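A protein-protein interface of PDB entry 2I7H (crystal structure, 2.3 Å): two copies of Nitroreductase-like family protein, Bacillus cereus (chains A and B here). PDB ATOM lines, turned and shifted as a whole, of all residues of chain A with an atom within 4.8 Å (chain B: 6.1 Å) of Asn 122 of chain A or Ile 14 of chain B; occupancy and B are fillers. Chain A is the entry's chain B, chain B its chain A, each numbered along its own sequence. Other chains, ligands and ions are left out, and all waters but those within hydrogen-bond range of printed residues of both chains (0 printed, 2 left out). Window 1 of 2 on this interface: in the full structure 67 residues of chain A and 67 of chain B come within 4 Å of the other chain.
NH2 of Arg 17 of chain B lies within hydrogen-bond range of O of Trp 42 of chain A, 3.4 Å away.
OE1 of Gln 121 of chain B sits close to OD1 of Asn 122 of chain A (2.9 Å).
The side-chain amino group of Lys 15 of chain B lies close to the backbone carbonyl oxygen of Ala 11 of chain B (3.5 Å).
The side-chain amide nitrogen (ND2) of Asn 122 of chain A lies within hydrogen-bond range of the backbone carbonyl oxygen (O) of Ala 40 of chain A, 3.2 Å away.
The side-chain hydroxyl (OG) of Ser 9 of chain B lies close to the backbone NH (N) of Ala 11 of chain B (3.2 Å).
CG2 of Ile 14 of chain B touches O of Asp 39 of chain A, at 3.6 Å.
OD1 of Asp 39 of chain A touches CD of Lys 15 of chain B (3.6 Å).
Trp 42 of chain A touches Ile 14 of chain B.
Ala 43 of chain A touches Arg 17 of chain B.
CB of Gln 121 of chain B touches CB of Ala 118 of chain A, 3.98 Å away.
Asn 122 of chain A touches Ile 14 of chain B (ND2 to CG2, 3.6 Å).
CD1 of Leu 125 of chain B touches OD1 of Asn 122 of chain A, 3.7 Å away.
Leu 125 of chain B touches Leu 125 of chain A (CD1 to CD1, 3.9 Å).
Ile 10 of chain B touches Leu 126 of chain A (CD1 to CA, 3.6 Å).
Ala 11 of chain B touches Leu 126 of chain A.
Asn 122 of chain A touches three residues of chain B.
Of the printed residues of chain A, Ile 10 of chain B touches Leu 125 and Leu 126.
Of the printed residues of chain A, Ala 11 of chain B touches Leu 126 (3.5 Å).
Of chain A, only Asp 39 (3.6 Å), Trp 42 (3.5 Å), Asn 122 (3.6 Å) and Leu 126 (3.7 Å) come within 4 Å of Ile 14 of chain B.
Of the printed residues of chain A, Lys 15 of chain B touches Asp 39 (3.6 Å) and Trp 42 (3.7 Å).
Of the printed residues of chain A, Leu 125 of chain B touches Asn 122 and Leu 125.
The nearest residue of chain A that does not touch Ile 14 of chain B is Leu 125 of chain A (4.7 Å).
The nearest printed residue of chain A that does not touch Leu 125 of chain B is Gln 121 of chain A (6.1 Å).
Of the 13 printed residues of chain A, 7 touch a printed residue of chain B.
Printed residues of chain A that touch a printed residue of chain B: Asp 39, Trp 42, Ala 43, Ala 118, Asn 122, Leu 125 and Leu 126.
Of the 12 printed residues of chain B, 8 touch a printed residue of chain A.
Among the printed residues, 16 pairs touch across the chains.
Among the printed residues, no Asp or Glu carboxylate lies within 4 Å of a Lys or Arg side-chain nitrogen of the other chain.
Leu 125 of chain B touches its own counterpart, Leu 125 of chain A.
2 positions are printed for both chains.
Of the 16 pairs that touch across the chains among the printed residues, 1 has its exchanged pair printed and touching as well.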
ATOM      1  N   ASP A  39       2.911  -8.836  -0.282  1.00  0.00           N
ATOM      2  CA  ASP A  39       1.898  -8.000   0.379  1.00  0.00           C
ATOM      3  C   ASP A  39       1.431  -6.861  -0.550  1.00  0.00           C
ATOM      4  O   ASP A  39       0.243  -6.542  -0.610  1.00  0.00           O
ATOM      5  CB  ASP A  39       2.399  -7.438   1.722  1.00  0.00           C
ATOM      6  CG  ASP A  39       2.660  -8.513   2.780  1.00  0.00           C
ATOM      7  OD1 ASP A  39       2.028  -9.593   2.763  1.00  0.00           O
ATOM      8  OD2 ASP A  39       3.525  -8.262   3.658  1.00  0.00           O
ATOM      9  N   ALA A  40       2.381  -6.279  -1.291  1.00  0.00           N
ATOM     10  CA  ALA A  40       2.129  -5.174  -2.206  1.00  0.00           C
ATOM     11  C   ALA A  40       1.159  -5.509  -3.319  1.00  0.00           C
ATOM     12  O   ALA A  40       0.457  -4.611  -3.783  1.00  0.00           O
ATOM     13  CB  ALA A  40       3.430  -4.622  -2.771  1.00  0.00           C
ATOM     14  N   TRP A  42      -1.601  -6.816  -3.271  1.00  0.00           N
ATOM     15  CA  TRP A  42      -2.969  -6.481  -2.900  1.00  0.00           C
ATOM     16  C   TRP A  42      -3.403  -5.056  -3.277  1.00  0.00           C
ATOM     17  O   TRP A  42      -4.363  -4.539  -2.700  1.00  0.00           O
ATOM     18  CB  TRP A  42      -3.254  -6.853  -1.415  1.00  0.00           C
ATOM     19  CG  TRP A  42      -3.222  -8.350  -1.237  1.00  0.00           C
ATOM     20  CD1 TRP A  42      -2.133  -9.112  -0.960  1.00  0.00           C
ATOM     21  CD2 TRP A  42      -4.317  -9.258  -1.402  1.00  0.00           C
ATOM     22  NE1 TRP A  42      -2.473 -10.454  -0.945  1.00  0.00           N
ATOM     23  CE2 TRP A  42      -3.811 -10.568  -1.206  1.00  0.00           C
ATOM     24  CE3 TRP A  42      -5.679  -9.096  -1.693  1.00  0.00           C
ATOM     25  CZ2 TRP A  42      -4.623 -11.704  -1.264  1.00  0.00           C
ATOM     26  CZ3 TRP A  42      -6.468 -10.204  -1.771  1.00  0.00           C
ATOM     27  CH2 TRP A  42      -5.932 -11.506  -1.561  1.00  0.00           C
ATOM     28  N   ALA A  43      -2.746  -4.441  -4.273  1.00  0.00           N
ATOM     29  CA  ALA A  43      -3.172  -3.150  -4.822  1.00  0.00           C
ATOM     30  C   ALA A  43      -4.432  -3.304  -5.662  1.00  0.00           C
ATOM     31  O   ALA A  43      -4.685  -4.382  -6.183  1.00  0.00           O
ATOM     32  CB  ALA A  43      -2.043  -2.483  -5.672  1.00  0.00           C
ATOM     33  N   ALA A 118       0.193   1.900  -7.783  1.00  0.00           N
ATOM     34  CA  ALA A 118      -0.418   1.557  -6.504  1.00  0.00           C
ATOM     35  C   ALA A 118       0.329   0.391  -5.789  1.00  0.00           C
ATOM     36  O   ALA A 118       0.553   0.438  -4.568  1.00  0.00           O
ATOM     37  CB  ALA A 118      -1.931   1.294  -6.681  1.00  0.00           C
ATOM     38  N   PHE A 119       0.723  -0.629  -6.547  1.00  0.00           N
ATOM     39  CA  PHE A 119       1.613  -1.704  -6.088  1.00  0.00           C
ATOM     40  C   PHE A 119       2.952  -1.131  -5.524  1.00  0.00           C
ATOM     41  O   PHE A 119       3.412  -1.528  -4.437  1.00  0.00           O
ATOM     42  CB  PHE A 119       1.845  -2.665  -7.289  1.00  0.00           C
ATOM     43  CG  PHE A 119       2.992  -3.582  -7.158  1.00  0.00           C
ATOM     44  CD1 PHE A 119       2.895  -4.733  -6.380  1.00  0.00           C
ATOM     45  CD2 PHE A 119       4.173  -3.359  -7.873  1.00  0.00           C
ATOM     46  CE1 PHE A 119       3.985  -5.616  -6.247  1.00  0.00           C
ATOM     47  CE2 PHE A 119       5.232  -4.256  -7.795  1.00  0.00           C
ATOM     48  CZ  PHE A 119       5.149  -5.392  -6.966  1.00  0.00           C
ATOM     49  N   MET A 120       3.546  -0.169  -6.233  1.00  0.00           N
ATOM     50  CA  MET A 120       4.814   0.405  -5.781  1.00  0.00           C
ATOM     51  C   MET A 120       4.677   1.256  -4.528  1.00  0.00           C
ATOM     52  O   MET A 120       5.496   1.112  -3.606  1.00  0.00           O
ATOM     53  CB  MET A 120       5.529   1.159  -6.898  1.00  0.00           C
ATOM     54  CG  MET A 120       5.902   0.263  -8.056  1.00  0.00           C
ATOM     55  SD  MET A 120       6.697   1.282  -9.554  1.00  0.00           S
ATOM     56  CE  MET A 120       8.481   1.557  -8.926  1.00  0.00           C
ATOM     57  N   GLN A 121       3.643   2.106  -4.468  1.00  0.00           N
ATOM     58  CA  GLN A 121       3.381   2.848  -3.233  1.00  0.00           C
ATOM     59  C   GLN A 121       3.102   1.893  -2.076  1.00  0.00           C
ATOM     60  O   GLN A 121       3.579   2.119  -0.984  1.00  0.00           O
ATOM     61  CB  GLN A 121       2.247   3.891  -3.400  1.00  0.00           C
ATOM     62  CG  GLN A 121       1.776   4.562  -2.144  1.00  0.00           C
ATOM     63  CD  GLN A 121       2.798   5.443  -1.448  1.00  0.00           C
ATOM     64  OE1 GLN A 121       2.445   6.166  -0.505  1.00  0.00           O
ATOM     65  NE2 GLN A 121       4.047   5.406  -1.886  1.00  0.00           N
ATOM     66  N   ASN A 122       2.372   0.807  -2.324  1.00  0.00           N
ATOM     67  CA  ASN A 122       2.165  -0.195  -1.285  1.00  0.00           C
ATOM     68  C   ASN A 122       3.483  -0.701  -0.768  1.00  0.00           C
ATOM     69  O   ASN A 122       3.698  -0.787   0.439  1.00  0.00           O
ATOM     70  CB  ASN A 122       1.363  -1.383  -1.779  1.00  0.00           C
ATOM     71  CG  ASN A 122      -0.111  -1.160  -1.711  1.00  0.00           C
ATOM     72  OD1 ASN A 122      -0.558  -0.236  -1.095  1.00  0.00           O
ATOM     73  ND2 ASN A 122      -0.866  -2.018  -2.344  1.00  0.00           N
ATOM     74  N   PHE A 123       4.365  -1.053  -1.692  1.00  0.00           N
ATOM     75  CA  PHE A 123       5.644  -1.594  -1.301  1.00  0.00           C
ATOM     76  C   PHE A 123       6.483  -0.606  -0.454  1.00  0.00           C
ATOM     77  O   PHE A 123       7.175  -1.027   0.451  1.00  0.00           O
ATOM     78  CB  PHE A 123       6.451  -2.004  -2.547  1.00  0.00           C
ATOM     79  CG  PHE A 123       7.792  -2.496  -2.213  1.00  0.00           C
ATOM     80  CD1 PHE A 123       7.968  -3.790  -1.813  1.00  0.00           C
ATOM     81  CD2 PHE A 123       8.903  -1.625  -2.222  1.00  0.00           C
ATOM     82  CE1 PHE A 123       9.248  -4.259  -1.473  1.00  0.00           C
ATOM     83  CE2 PHE A 123      10.163  -2.079  -1.866  1.00  0.00           C
ATOM     84  CZ  PHE A 123      10.329  -3.382  -1.492  1.00  0.00           C
ATOM     85  N   GLN A 124       6.461   0.678  -0.801  1.00  0.00           N
ATOM     86  CA  GLN A 124       7.163   1.704  -0.057  1.00  0.00           C
ATOM     87  C   GLN A 124       6.722   1.742   1.413  1.00  0.00           C
ATOM     88  O   GLN A 124       7.555   1.836   2.316  1.00  0.00           O
ATOM     89  CB  GLN A 124       7.015   3.108  -0.724  1.00  0.00           C
ATOM     90  CG  GLN A 124       7.649   3.202  -2.150  1.00  0.00           C
ATOM     91  CD  GLN A 124       7.948   4.625  -2.570  1.00  0.00           C
ATOM     92  OE1 GLN A 124       7.086   5.518  -2.491  1.00  0.00           O
ATOM     93  NE2 GLN A 124       9.173   4.863  -2.985  1.00  0.00           N
ATOM     94  N   LEU A 125       5.418   1.668   1.635  1.00  0.00           N
ATOM     95  CA  LEU A 125       4.828   1.747   2.971  1.00  0.00           C
ATOM     96  C   LEU A 125       5.072   0.462   3.755  1.00  0.00           C
ATOM     97  O   LEU A 125       5.369   0.484   4.939  1.00  0.00           O
ATOM     98  CB  LEU A 125       3.319   2.004   2.858  1.00  0.00           C
ATOM     99  CG  LEU A 125       2.889   3.276   2.115  1.00  0.00           C
ATOM    100  CD1 LEU A 125       1.316   3.266   1.745  1.00  0.00           C
ATOM    101  CD2 LEU A 125       3.302   4.523   2.892  1.00  0.00           C
ATOM    102  N   LEU A 126       4.934  -0.662   3.071  1.00  0.00           N
ATOM    103  CA  LEU A 126       5.238  -1.973   3.633  1.00  0.00           C
ATOM    104  C   LEU A 126       6.688  -2.031   4.097  1.00  0.00           C
ATOM    105  O   LEU A 126       6.980  -2.524   5.182  1.00  0.00           O
ATOM    106  CB  LEU A 126       4.957  -3.055   2.585  1.00  0.00           C
ATOM    107  CG  LEU A 126       3.496  -3.492   2.373  1.00  0.00           C
ATOM    108  CD1 LEU A 126       3.373  -4.334   1.087  1.00  0.00           C
ATOM    109  CD2 LEU A 126       2.937  -4.304   3.607  1.00  0.00           C
ATOM    110  N   SER B   9      -0.472  -3.504  11.792  1.00  0.00           N
ATOM    111  CA  SER B   9       0.430  -3.480  10.622  1.00  0.00           C
ATOM    112  C   SER B   9      -0.308  -2.904   9.413  1.00  0.00           C
ATOM    113  O   SER B   9      -1.455  -3.296   9.148  1.00  0.00           O
ATOM    114  CB  SER B   9       0.930  -4.914  10.334  1.00  0.00           C
ATOM    115  OG  SER B   9       1.693  -5.017   9.135  1.00  0.00           O
ATOM    116  N   ILE B  10       0.335  -1.992   8.692  1.00  0.00           N
ATOM    117  CA  ILE B  10      -0.239  -1.434   7.471  1.00  0.00           C
ATOM    118  C   ILE B  10      -0.396  -2.502   6.393  1.00  0.00           C
ATOM    119  O   ILE B  10      -1.176  -2.336   5.460  1.00  0.00           O
ATOM    120  CB  ILE B  10       0.542  -0.168   6.967  1.00  0.00           C
ATOM    121  CG1 ILE B  10       1.477  -0.451   5.778  1.00  0.00           C
ATOM    122  CG2 ILE B  10       1.246   0.494   8.119  1.00  0.00           C
ATOM    123  CD1 ILE B  10       2.775  -1.107   6.124  1.00  0.00           C
ATOM    124  N   ALA B  11       0.344  -3.600   6.548  1.00  0.00           N
ATOM    125  CA  ALA B  11       0.165  -4.809   5.744  1.00  0.00           C
ATOM    126  C   ALA B  11      -1.279  -5.314   5.841  1.00  0.00           C
ATOM    127  O   ALA B  11      -1.872  -5.758   4.845  1.00  0.00           O
ATOM    128  CB  ALA B  11       1.138  -5.893   6.197  1.00  0.00           C
ATOM    129  N   ASN B  12      -1.855  -5.248   7.037  1.00  0.00           N
ATOM    130  CA  ASN B  12      -3.214  -5.735   7.219  1.00  0.00           C
ATOM    131  C   ASN B  12      -4.221  -4.895   6.466  1.00  0.00           C
ATOM    132  O   ASN B  12      -5.052  -5.433   5.739  1.00  0.00           O
ATOM    133  CB  ASN B  12      -3.574  -5.889   8.698  1.00  0.00           C
ATOM    134  CG  ASN B  12      -2.911  -7.091   9.321  1.00  0.00           C
ATOM    135  OD1 ASN B  12      -2.522  -8.028   8.630  1.00  0.00           O
ATOM    136  ND2 ASN B  12      -2.781  -7.077  10.632  1.00  0.00           N
ATOM    137  N   VAL B  13      -4.111  -3.579   6.602  1.00  0.00           N
ATOM    138  CA  VAL B  13      -4.973  -2.650   5.876  1.00  0.00           C
ATOM    139  C   VAL B  13      -4.860  -2.841   4.351  1.00  0.00           C
ATOM    140  O   VAL B  13      -5.892  -2.971   3.654  1.00  0.00           O
ATOM    141  CB  VAL B  13      -4.653  -1.193   6.291  1.00  0.00           C
ATOM    142  CG1 VAL B  13      -5.545  -0.208   5.570  1.00  0.00           C
ATOM    143  CG2 VAL B  13      -4.802  -1.045   7.834  1.00  0.00           C
ATOM    144  N   ILE B  14      -3.617  -2.887   3.851  1.00  0.00           N
ATOM    145  CA  ILE B  14      -3.340  -3.098   2.424  1.00  0.00           C
ATOM    146  C   ILE B  14      -4.014  -4.380   1.894  1.00  0.00           C
ATOM    147  O   ILE B  14      -4.616  -4.384   0.823  1.00  0.00           O
ATOM    148  CB  ILE B  14      -1.808  -3.137   2.133  1.00  0.00           C
ATOM    149  CG1 ILE B  14      -1.210  -1.722   2.280  1.00  0.00           C
ATOM    150  CG2 ILE B  14      -1.533  -3.756   0.784  1.00  0.00           C
ATOM    151  CD1 ILE B  14       0.300  -1.595   2.172  1.00  0.00           C
ATOM    152  N   LYS B  15      -3.910  -5.462   2.648  1.00  0.00           N
ATOM    153  CA  LYS B  15      -4.481  -6.740   2.217  1.00  0.00           C
ATOM    154  C   LYS B  15      -5.982  -6.901   2.459  1.00  0.00           C
ATOM    155  O   LYS B  15      -6.636  -7.722   1.797  1.00  0.00           O
ATOM    156  CB  LYS B  15      -3.725  -7.906   2.845  1.00  0.00           C
ATOM    157  CG  LYS B  15      -2.213  -7.890   2.577  1.00  0.00           C
ATOM    158  CD  LYS B  15      -1.589  -9.258   2.837  1.00  0.00           C
ATOM    159  CE  LYS B  15      -1.971  -9.806   4.210  1.00  0.00           C
ATOM    160  NZ  LYS B  15      -1.199  -9.145   5.303  1.00  0.00           N
ATOM    161  N   GLU B  16      -6.534  -6.125   3.382  1.00  0.00           N
ATOM    162  CA  GLU B  16      -7.938  -6.260   3.740  1.00  0.00           C
ATOM    163  C   GLU B  16      -8.821  -5.286   2.953  1.00  0.00           C
ATOM    164  O   GLU B  16      -9.974  -5.587   2.679  1.00  0.00           O
ATOM    165  CB  GLU B  16      -8.125  -6.115   5.259  1.00  0.00           C
ATOM    166  CG  GLU B  16      -7.630  -7.327   6.061  1.00  0.00           C
ATOM    167  CD  GLU B  16      -7.718  -7.154   7.590  1.00  0.00           C
ATOM    168  OE1 GLU B  16      -8.243  -6.112   8.063  1.00  0.00           O
ATOM    169  OE2 GLU B  16      -7.270  -8.074   8.330  1.00  0.00           O
ATOM    170  N   ARG B  17      -8.270  -4.129   2.590  1.00  0.00           N
ATOM    171  CA  ARG B  17      -8.931  -3.183   1.680  1.00  0.00           C
ATOM    172  C   ARG B  17      -9.594  -3.888   0.501  1.00  0.00           C
ATOM    173  O   ARG B  17      -8.985  -4.727  -0.167  1.00  0.00           O
ATOM    174  CB  ARG B  17      -7.918  -2.138   1.151  1.00  0.00           C
ATOM    175  CG  ARG B  17      -8.525  -0.996   0.326  1.00  0.00           C
ATOM    176  CD  ARG B  17      -7.594  -0.530  -0.849  1.00  0.00           C
ATOM    177  NE  ARG B  17      -7.194  -1.643  -1.729  1.00  0.00           N
ATOM    178  CZ  ARG B  17      -7.904  -2.148  -2.749  1.00  0.00           C
ATOM    179  NH1 ARG B  17      -9.098  -1.666  -3.070  1.00  0.00           N
ATOM    180  NH2 ARG B  17      -7.430  -3.188  -3.444  1.00  0.00           N
ATOM    181  N   ARG B  18     -10.861  -3.555   0.281  1.00  0.00           N
ATOM    182  CA  ARG B  18     -11.615  -4.032  -0.871  1.00  0.00           C
ATOM    183  C   ARG B  18     -12.249  -2.837  -1.554  1.00  0.00           C
ATOM    184  O   ARG B  18     -12.649  -1.874  -0.890  1.00  0.00           O
ATOM    185  CB  ARG B  18     -12.750  -4.985  -0.449  1.00  0.00           C
ATOM    186  CG  ARG B  18     -12.369  -6.226   0.334  1.00  0.00           C
ATOM    187  CD  ARG B  18     -11.877  -7.325  -0.585  1.00  0.00           C
ATOM    188  NE  ARG B  18     -10.429  -7.229  -0.591  1.00  0.00           N
ATOM    189  CZ  ARG B  18      -9.619  -7.950   0.178  1.00  0.00           C
ATOM    190  NH1 ARG B  18     -10.088  -8.912   0.980  1.00  0.00           N
ATOM    191  NH2 ARG B  18      -8.331  -7.713   0.107  1.00  0.00           N
ATOM    192  N   GLN B 121      -4.177   5.748  -3.862  1.00  0.00           N
ATOM    193  CA  GLN B 121      -3.974   4.539  -3.109  1.00  0.00           C
ATOM    194  C   GLN B 121      -3.811   4.821  -1.606  1.00  0.00           C
ATOM    195  O   GLN B 121      -4.428   4.143  -0.794  1.00  0.00           O
ATOM    196  CB  GLN B 121      -2.790   3.736  -3.652  1.00  0.00           C
ATOM    197  CG  GLN B 121      -2.419   2.527  -2.785  1.00  0.00           C
ATOM    198  CD  GLN B 121      -3.472   1.439  -2.727  1.00  0.00           C
ATOM    199  OE1 GLN B 121      -3.248   0.388  -2.108  1.00  0.00           O
ATOM    200  NE2 GLN B 121      -4.621   1.673  -3.339  1.00  0.00           N
ATOM    201  N   LEU B 125      -6.386   3.505   1.425  1.00  0.00           N
ATOM    202  CA  LEU B 125      -5.878   2.871   2.641  1.00  0.00           C
ATOM    203  C   LEU B 125      -6.320   3.606   3.904  1.00  0.00           C
ATOM    204  O   LEU B 125      -6.874   3.018   4.821  1.00  0.00           O
ATOM    205  CB  LEU B 125      -4.338   2.769   2.578  1.00  0.00           C
ATOM    206  CG  LEU B 125      -3.799   1.831   1.509  1.00  0.00           C
ATOM    207  CD1 LEU B 125      -2.250   1.821   1.471  1.00  0.00           C
ATOM    208  CD2 LEU B 125      -4.391   0.437   1.698  1.00  0.00           C
